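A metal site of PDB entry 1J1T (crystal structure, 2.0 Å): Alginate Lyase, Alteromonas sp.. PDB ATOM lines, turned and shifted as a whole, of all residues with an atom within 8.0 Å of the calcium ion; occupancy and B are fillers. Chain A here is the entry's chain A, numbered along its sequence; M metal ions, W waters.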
ATOM      1  N   ASP A  82       1.365 -27.597  10.536  1.00  0.00           N
ATOM      2  CA  ASP A  82       0.457 -26.809  11.355  1.00  0.00           C
ATOM      3  C   ASP A  82      -0.757 -26.439  10.504  1.00  0.00           C
ATOM      4  O   ASP A  82      -0.619 -26.141   9.322  1.00  0.00           O
ATOM      5  CB  ASP A  82       1.118 -25.513  11.827  1.00  0.00           C
ATOM      6  CG  ASP A  82       2.309 -25.753  12.742  1.00  0.00           C
ATOM      7  OD1 ASP A  82       3.017 -24.763  13.042  1.00  0.00           O
ATOM      8  OD2 ASP A  82       2.542 -26.909  13.157  1.00  0.00           O
ATOM      9  N   GLY A  83      -1.944 -26.450  11.102  1.00  0.00           N
ATOM     10  CA  GLY A  83      -3.143 -26.076  10.366  1.00  0.00           C
ATOM     11  C   GLY A  83      -3.826 -27.197   9.601  1.00  0.00           C
ATOM     12  O   GLY A  83      -4.918 -27.022   9.069  1.00  0.00           O
ATOM     13  N   GLY A  84      -3.170 -28.353   9.539  1.00  0.00           N
ATOM     14  CA  GLY A  84      -3.737 -29.479   8.830  1.00  0.00           C
ATOM     15  C   GLY A  84      -4.936 -30.091   9.519  1.00  0.00           C
ATOM     16  O   GLY A  84      -5.077 -30.032  10.744  1.00  0.00           O
ATOM     17  N   SER A 105      -7.196 -32.560  13.783  1.00  0.00           N
ATOM     18  CA  SER A 105      -7.138 -31.250  13.161  1.00  0.00           C
ATOM     19  C   SER A 105      -6.587 -30.130  14.013  1.00  0.00           C
ATOM     20  O   SER A 105      -6.735 -30.107  15.244  1.00  0.00           O
ATOM     21  CB  SER A 105      -8.519 -30.852  12.631  1.00  0.00           C
ATOM     22  OG  SER A 105      -9.315 -30.260  13.645  1.00  0.00           O
ATOM     23  N   ASP A 106      -5.955 -29.178  13.331  1.00  0.00           N
ATOM     24  CA  ASP A 106      -5.330 -28.034  13.947  1.00  0.00           C
ATOM     25  C   ASP A 106      -6.061 -26.773  13.503  1.00  0.00           C
ATOM     26  O   ASP A 106      -5.463 -25.882  12.901  1.00  0.00           O
ATOM     27  CB  ASP A 106      -3.853 -28.020  13.522  1.00  0.00           C
ATOM     28  CG  ASP A 106      -3.061 -26.900  14.170  1.00  0.00           C
ATOM     29  OD1 ASP A 106      -3.562 -26.327  15.141  1.00  0.00           O
ATOM     30  OD2 ASP A 106      -1.934 -26.615  13.722  1.00  0.00           O
ATOM     31  N   THR A 107      -7.361 -26.704  13.780  1.00  0.00           N
ATOM     32  CA  THR A 107      -8.171 -25.550  13.391  1.00  0.00           C
ATOM     33  C   THR A 107      -8.675 -24.763  14.605  1.00  0.00           C
ATOM     34  O   THR A 107      -8.378 -25.085  15.752  1.00  0.00           O
ATOM     35  CB  THR A 107      -9.418 -25.952  12.570  1.00  0.00           C
ATOM     36  OG1 THR A 107     -10.402 -26.529  13.442  1.00  0.00           O
ATOM     37  CG2 THR A 107      -9.050 -26.962  11.490  1.00  0.00           C
ATOM     38  N   ASP A 108      -9.468 -23.732  14.307  1.00  0.00           N
ATOM     39  CA  ASP A 108     -10.039 -22.861  15.327  1.00  0.00           C
ATOM     40  C   ASP A 108     -11.454 -23.274  15.722  1.00  0.00           C
ATOM     41  O   ASP A 108     -12.111 -22.567  16.480  1.00  0.00           O
ATOM     42  CB  ASP A 108     -10.047 -21.422  14.829  1.00  0.00           C
ATOM     43  CG  ASP A 108      -9.590 -20.431  15.884  1.00  0.00           C
ATOM     44  OD1 ASP A 108      -8.437 -20.563  16.362  1.00  0.00           O
ATOM     45  OD2 ASP A 108     -10.374 -19.529  16.242  1.00  0.00           O
ATOM     46  N   GLU A 109     -11.933 -24.416  15.225  1.00  0.00           N
ATOM     47  CA  GLU A 109     -13.276 -24.862  15.593  1.00  0.00           C
ATOM     48  C   GLU A 109     -13.314 -25.046  17.103  1.00  0.00           C
ATOM     49  O   GLU A 109     -12.484 -25.746  17.670  1.00  0.00           O
ATOM     50  CB  GLU A 109     -13.645 -26.179  14.894  1.00  0.00           C
ATOM     51  CG  GLU A 109     -15.036 -26.675  15.285  1.00  0.00           C
ATOM     52  CD  GLU A 109     -15.461 -27.941  14.554  1.00  0.00           C
ATOM     53  OE1 GLU A 109     -16.439 -28.573  15.017  1.00  0.00           O
ATOM     54  OE2 GLU A 109     -14.838 -28.304  13.537  1.00  0.00           O
ATOM     55  N   ASN A 113     -10.267 -29.695  23.244  1.00  0.00           N
ATOM     56  CA  ASN A 113      -9.256 -29.385  24.246  1.00  0.00           C
ATOM     57  C   ASN A 113      -8.345 -28.223  23.891  1.00  0.00           C
ATOM     58  O   ASN A 113      -7.947 -27.466  24.781  1.00  0.00           O
ATOM     59  CB  ASN A 113      -8.406 -30.625  24.550  1.00  0.00           C
ATOM     60  CG  ASN A 113      -9.208 -31.731  25.188  1.00  0.00           C
ATOM     61  OD1 ASN A 113     -10.406 -31.591  25.450  1.00  0.00           O
ATOM     62  ND2 ASN A 113      -8.557 -32.860  25.459  1.00  0.00           N
ATOM     63  N   ASP A 114      -7.997 -28.083  22.612  1.00  0.00           N
ATOM     64  CA  ASP A 114      -7.125 -26.997  22.198  1.00  0.00           C
ATOM     65  C   ASP A 114      -7.930 -25.940  21.434  1.00  0.00           C
ATOM     66  O   ASP A 114      -8.013 -24.789  21.867  1.00  0.00           O
ATOM     67  CB  ASP A 114      -5.996 -27.536  21.316  1.00  0.00           C
ATOM     68  CG  ASP A 114      -4.979 -26.463  20.962  1.00  0.00           C
ATOM     69  OD1 ASP A 114      -4.124 -26.126  21.797  1.00  0.00           O
ATOM     70  OD2 ASP A 114      -5.049 -25.941  19.840  1.00  0.00           O
ATOM     71  N   SER A 115      -8.489 -26.326  20.297  1.00  0.00           N
ATOM     72  CA  SER A 115      -9.298 -25.438  19.485  1.00  0.00           C
ATOM     73  C   SER A 115      -8.612 -24.145  19.048  1.00  0.00           C
ATOM     74  O   SER A 115      -9.280 -23.124  18.876  1.00  0.00           O
ATOM     75  CB  SER A 115     -10.606 -25.092  20.209  1.00  0.00           C
ATOM     76  OG  SER A 115     -11.459 -26.221  20.294  1.00  0.00           O
ATOM     77  N   VAL A 116      -7.291 -24.175  18.882  1.00  0.00           N
ATOM     78  CA  VAL A 116      -6.558 -22.986  18.450  1.00  0.00           C
ATOM     79  C   VAL A 116      -5.978 -23.254  17.064  1.00  0.00           C
ATOM     80  O   VAL A 116      -5.080 -24.062  16.918  1.00  0.00           O
ATOM     81  CB  VAL A 116      -5.386 -22.660  19.392  1.00  0.00           C
ATOM     82  CG1 VAL A 116      -4.643 -21.438  18.876  1.00  0.00           C
ATOM     83  CG2 VAL A 116      -5.902 -22.430  20.808  1.00  0.00           C
ATOM     84  N   ALA A 117      -6.455 -22.553  16.062  1.00  0.00           N
ATOM     85  CA  ALA A 117      -5.976 -22.772  14.702  1.00  0.00           C
ATOM     86  C   ALA A 117      -4.473 -22.614  14.472  1.00  0.00           C
ATOM     87  O   ALA A 117      -3.813 -21.772  15.078  1.00  0.00           O
ATOM     88  CB  ALA A 117      -6.721 -21.868  13.735  1.00  0.00           C
ATOM     89  N   ASN A 118      -3.932 -23.466  13.595  1.00  0.00           N
ATOM     90  CA  ASN A 118      -2.547 -23.389  13.169  1.00  0.00           C
ATOM     91  C   ASN A 118      -1.453 -23.221  14.236  1.00  0.00           C
ATOM     92  O   ASN A 118      -0.520 -22.438  14.039  1.00  0.00           O
ATOM     93  CB  ASN A 118      -2.459 -22.218  12.159  1.00  0.00           C
ATOM     94  CG  ASN A 118      -1.226 -22.286  11.289  1.00  0.00           C
ATOM     95  OD1 ASN A 118      -0.944 -23.308  10.661  1.00  0.00           O
ATOM     96  ND2 ASN A 118      -0.496 -21.174  11.212  1.00  0.00           N
ATOM     97  N   ASN A 119      -1.549 -23.959  15.343  1.00  0.00           N
ATOM     98  CA  ASN A 119      -0.522 -23.834  16.383  1.00  0.00           C
ATOM     99  C   ASN A 119       0.261 -25.131  16.602  1.00  0.00           C
ATOM    100  O   ASN A 119       1.028 -25.253  17.546  1.00  0.00           O
ATOM    101  CB  ASN A 119      -1.145 -23.361  17.706  1.00  0.00           C
ATOM    102  CG  ASN A 119      -1.905 -24.463  18.429  1.00  0.00           C
ATOM    103  OD1 ASN A 119      -2.110 -25.546  17.882  1.00  0.00           O
ATOM    104  ND2 ASN A 119      -2.326 -24.184  19.661  1.00  0.00           N
ATOM    105  N   GLY A 120       0.065 -26.110  15.713  1.00  0.00           N
ATOM    106  CA  GLY A 120       0.793 -27.362  15.845  1.00  0.00           C
ATOM    107  C   GLY A 120       0.263 -28.375  16.837  1.00  0.00           C
ATOM    108  O   GLY A 120       0.799 -29.472  16.960  1.00  0.00           O
ATOM    109  N   ILE A 121      -0.786 -28.012  17.572  1.00  0.00           N
ATOM    110  CA  ILE A 121      -1.384 -28.940  18.537  1.00  0.00           C
ATOM    111  C   ILE A 121      -2.683 -29.424  17.905  1.00  0.00           C
ATOM    112  O   ILE A 121      -3.631 -28.666  17.799  1.00  0.00           O
ATOM    113  CB  ILE A 121      -1.679 -28.237  19.880  1.00  0.00           C
ATOM    114  CG1 ILE A 121      -0.356 -27.789  20.527  1.00  0.00           C
ATOM    115  CG2 ILE A 121      -2.454 -29.170  20.806  1.00  0.00           C
ATOM    116  CD1 ILE A 121      -0.528 -27.036  21.824  1.00  0.00           C
ATOM    117  N   PHE A 122      -2.730 -30.675  17.466  1.00  0.00           N
ATOM    118  CA  PHE A 122      -3.936 -31.174  16.831  1.00  0.00           C
ATOM    119  C   PHE A 122      -4.956 -31.749  17.794  1.00  0.00           C
ATOM    120  O   PHE A 122      -4.615 -32.512  18.699  1.00  0.00           O
ATOM    121  CB  PHE A 122      -3.607 -32.253  15.784  1.00  0.00           C
ATOM    122  CG  PHE A 122      -2.643 -31.792  14.732  1.00  0.00           C
ATOM    123  CD1 PHE A 122      -1.286 -31.706  15.018  1.00  0.00           C
ATOM    124  CD2 PHE A 122      -3.098 -31.391  13.491  1.00  0.00           C
ATOM    125  CE1 PHE A 122      -0.384 -31.218  14.063  1.00  0.00           C
ATOM    126  CE2 PHE A 122      -2.213 -30.895  12.527  1.00  0.00           C
ATOM    127  CZ  PHE A 122      -0.856 -30.809  12.813  1.00  0.00           C
ATOM    128  N   ASP A 123      -6.212 -31.360  17.598  1.00  0.00           N
ATOM    129  CA  ASP A 123      -7.296 -31.875  18.410  1.00  0.00           C
ATOM    130  C   ASP A 123      -7.704 -33.199  17.758  1.00  0.00           C
ATOM    131  O   ASP A 123      -7.754 -33.296  16.536  1.00  0.00           O
ATOM    132  CB  ASP A 123      -8.504 -30.945  18.370  1.00  0.00           C
ATOM    133  CG  ASP A 123      -8.295 -29.677  19.167  1.00  0.00           C
ATOM    134  OD1 ASP A 123      -8.079 -29.772  20.390  1.00  0.00           O
ATOM    135  OD2 ASP A 123      -8.332 -28.586  18.555  1.00  0.00           O
ATOM    136  N   THR A 142      -5.383 -34.514  22.424  1.00  0.00           N
ATOM    137  CA  THR A 142      -4.575 -33.631  21.579  1.00  0.00           C
ATOM    138  C   THR A 142      -3.222 -34.283  21.359  1.00  0.00           C
ATOM    139  O   THR A 142      -2.793 -35.139  22.131  1.00  0.00           O
ATOM    140  CB  THR A 142      -4.302 -32.251  22.236  1.00  0.00           C
ATOM    141  OG1 THR A 142      -3.631 -32.442  23.486  1.00  0.00           O
ATOM    142  CG2 THR A 142      -5.600 -31.490  22.450  1.00  0.00           C
ATOM    143  N   MET A 143      -2.539 -33.859  20.297  1.00  0.00           N
ATOM    144  CA  MET A 143      -1.226 -34.409  19.986  1.00  0.00           C
ATOM    145  C   MET A 143      -0.470 -33.424  19.120  1.00  0.00           C
ATOM    146  O   MET A 143      -1.057 -32.554  18.500  1.00  0.00           O
ATOM    147  CB  MET A 143      -1.375 -35.736  19.234  1.00  0.00           C
ATOM    148  CG  MET A 143      -1.930 -35.573  17.808  1.00  0.00           C
ATOM    149  SD  MET A 143      -2.348 -37.137  17.009  1.00  0.00           S
ATOM    150  CE  MET A 143      -0.704 -37.859  16.800  1.00  0.00           C
ATOM    151  N   PRO A 192      -7.725 -23.257   8.330  1.00  0.00           N
ATOM    152  CA  PRO A 192      -7.806 -23.558   9.773  1.00  0.00           C
ATOM    153  C   PRO A 192      -8.370 -22.437  10.629  1.00  0.00           C
ATOM    154  O   PRO A 192      -8.926 -22.681  11.701  1.00  0.00           O
ATOM    155  CB  PRO A 192      -6.360 -23.899  10.114  1.00  0.00           C
ATOM    156  CG  PRO A 192      -5.584 -22.984   9.220  1.00  0.00           C
ATOM    157  CD  PRO A 192      -6.325 -23.131   7.895  1.00  0.00           C
HETATM  158 CA    CA M   1      -4.535 -26.411  17.450  1.00  0.00          CA
HETATM  159  O   HOH W   1      -7.048 -26.934  16.929  1.00  0.00           O
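Within 4 Å of the calcium ion: Asp 106, Asp 114, Val 116, Asn 119 and Ile 121.
Water W1 lies within hydrogen-bond range of the backbone carbonyl oxygen of Thr 107 (2.6 Å), the side-chain carboxylate of Asp 123 (2.6 Å) and the backbone NH of Val 116 (3.4 Å).
The calcium ion is bound by O of Ile 121, O of Val 116, OD2 of Asp 114, OD1 of Asp 106, OD1 of Asn 119 and water W1.
N of Val 116 sits close to O of Thr 107.
The backbone NH (N) of Asp 114 lies within hydrogen-bond range of the side-chain carboxylate (OD1) of Asp 123 (2.8 Å).
O of Asp 106 lies within hydrogen-bond range of N of Asn 118 (2.9 Å).
OD2 of Asp 106 sits at hydrogen-bond distance from N of Gly 120 (2.9 Å).
The backbone NH (N) of Gly 83 sits at hydrogen-bond distance from the side-chain carboxylate (OD2) of Asp 106 (2.6 Å).
The backbone NH (N) of Asp 106 lies within hydrogen-bond range of the backbone carbonyl oxygen (O) of Gly 84, at 2.9 Å.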
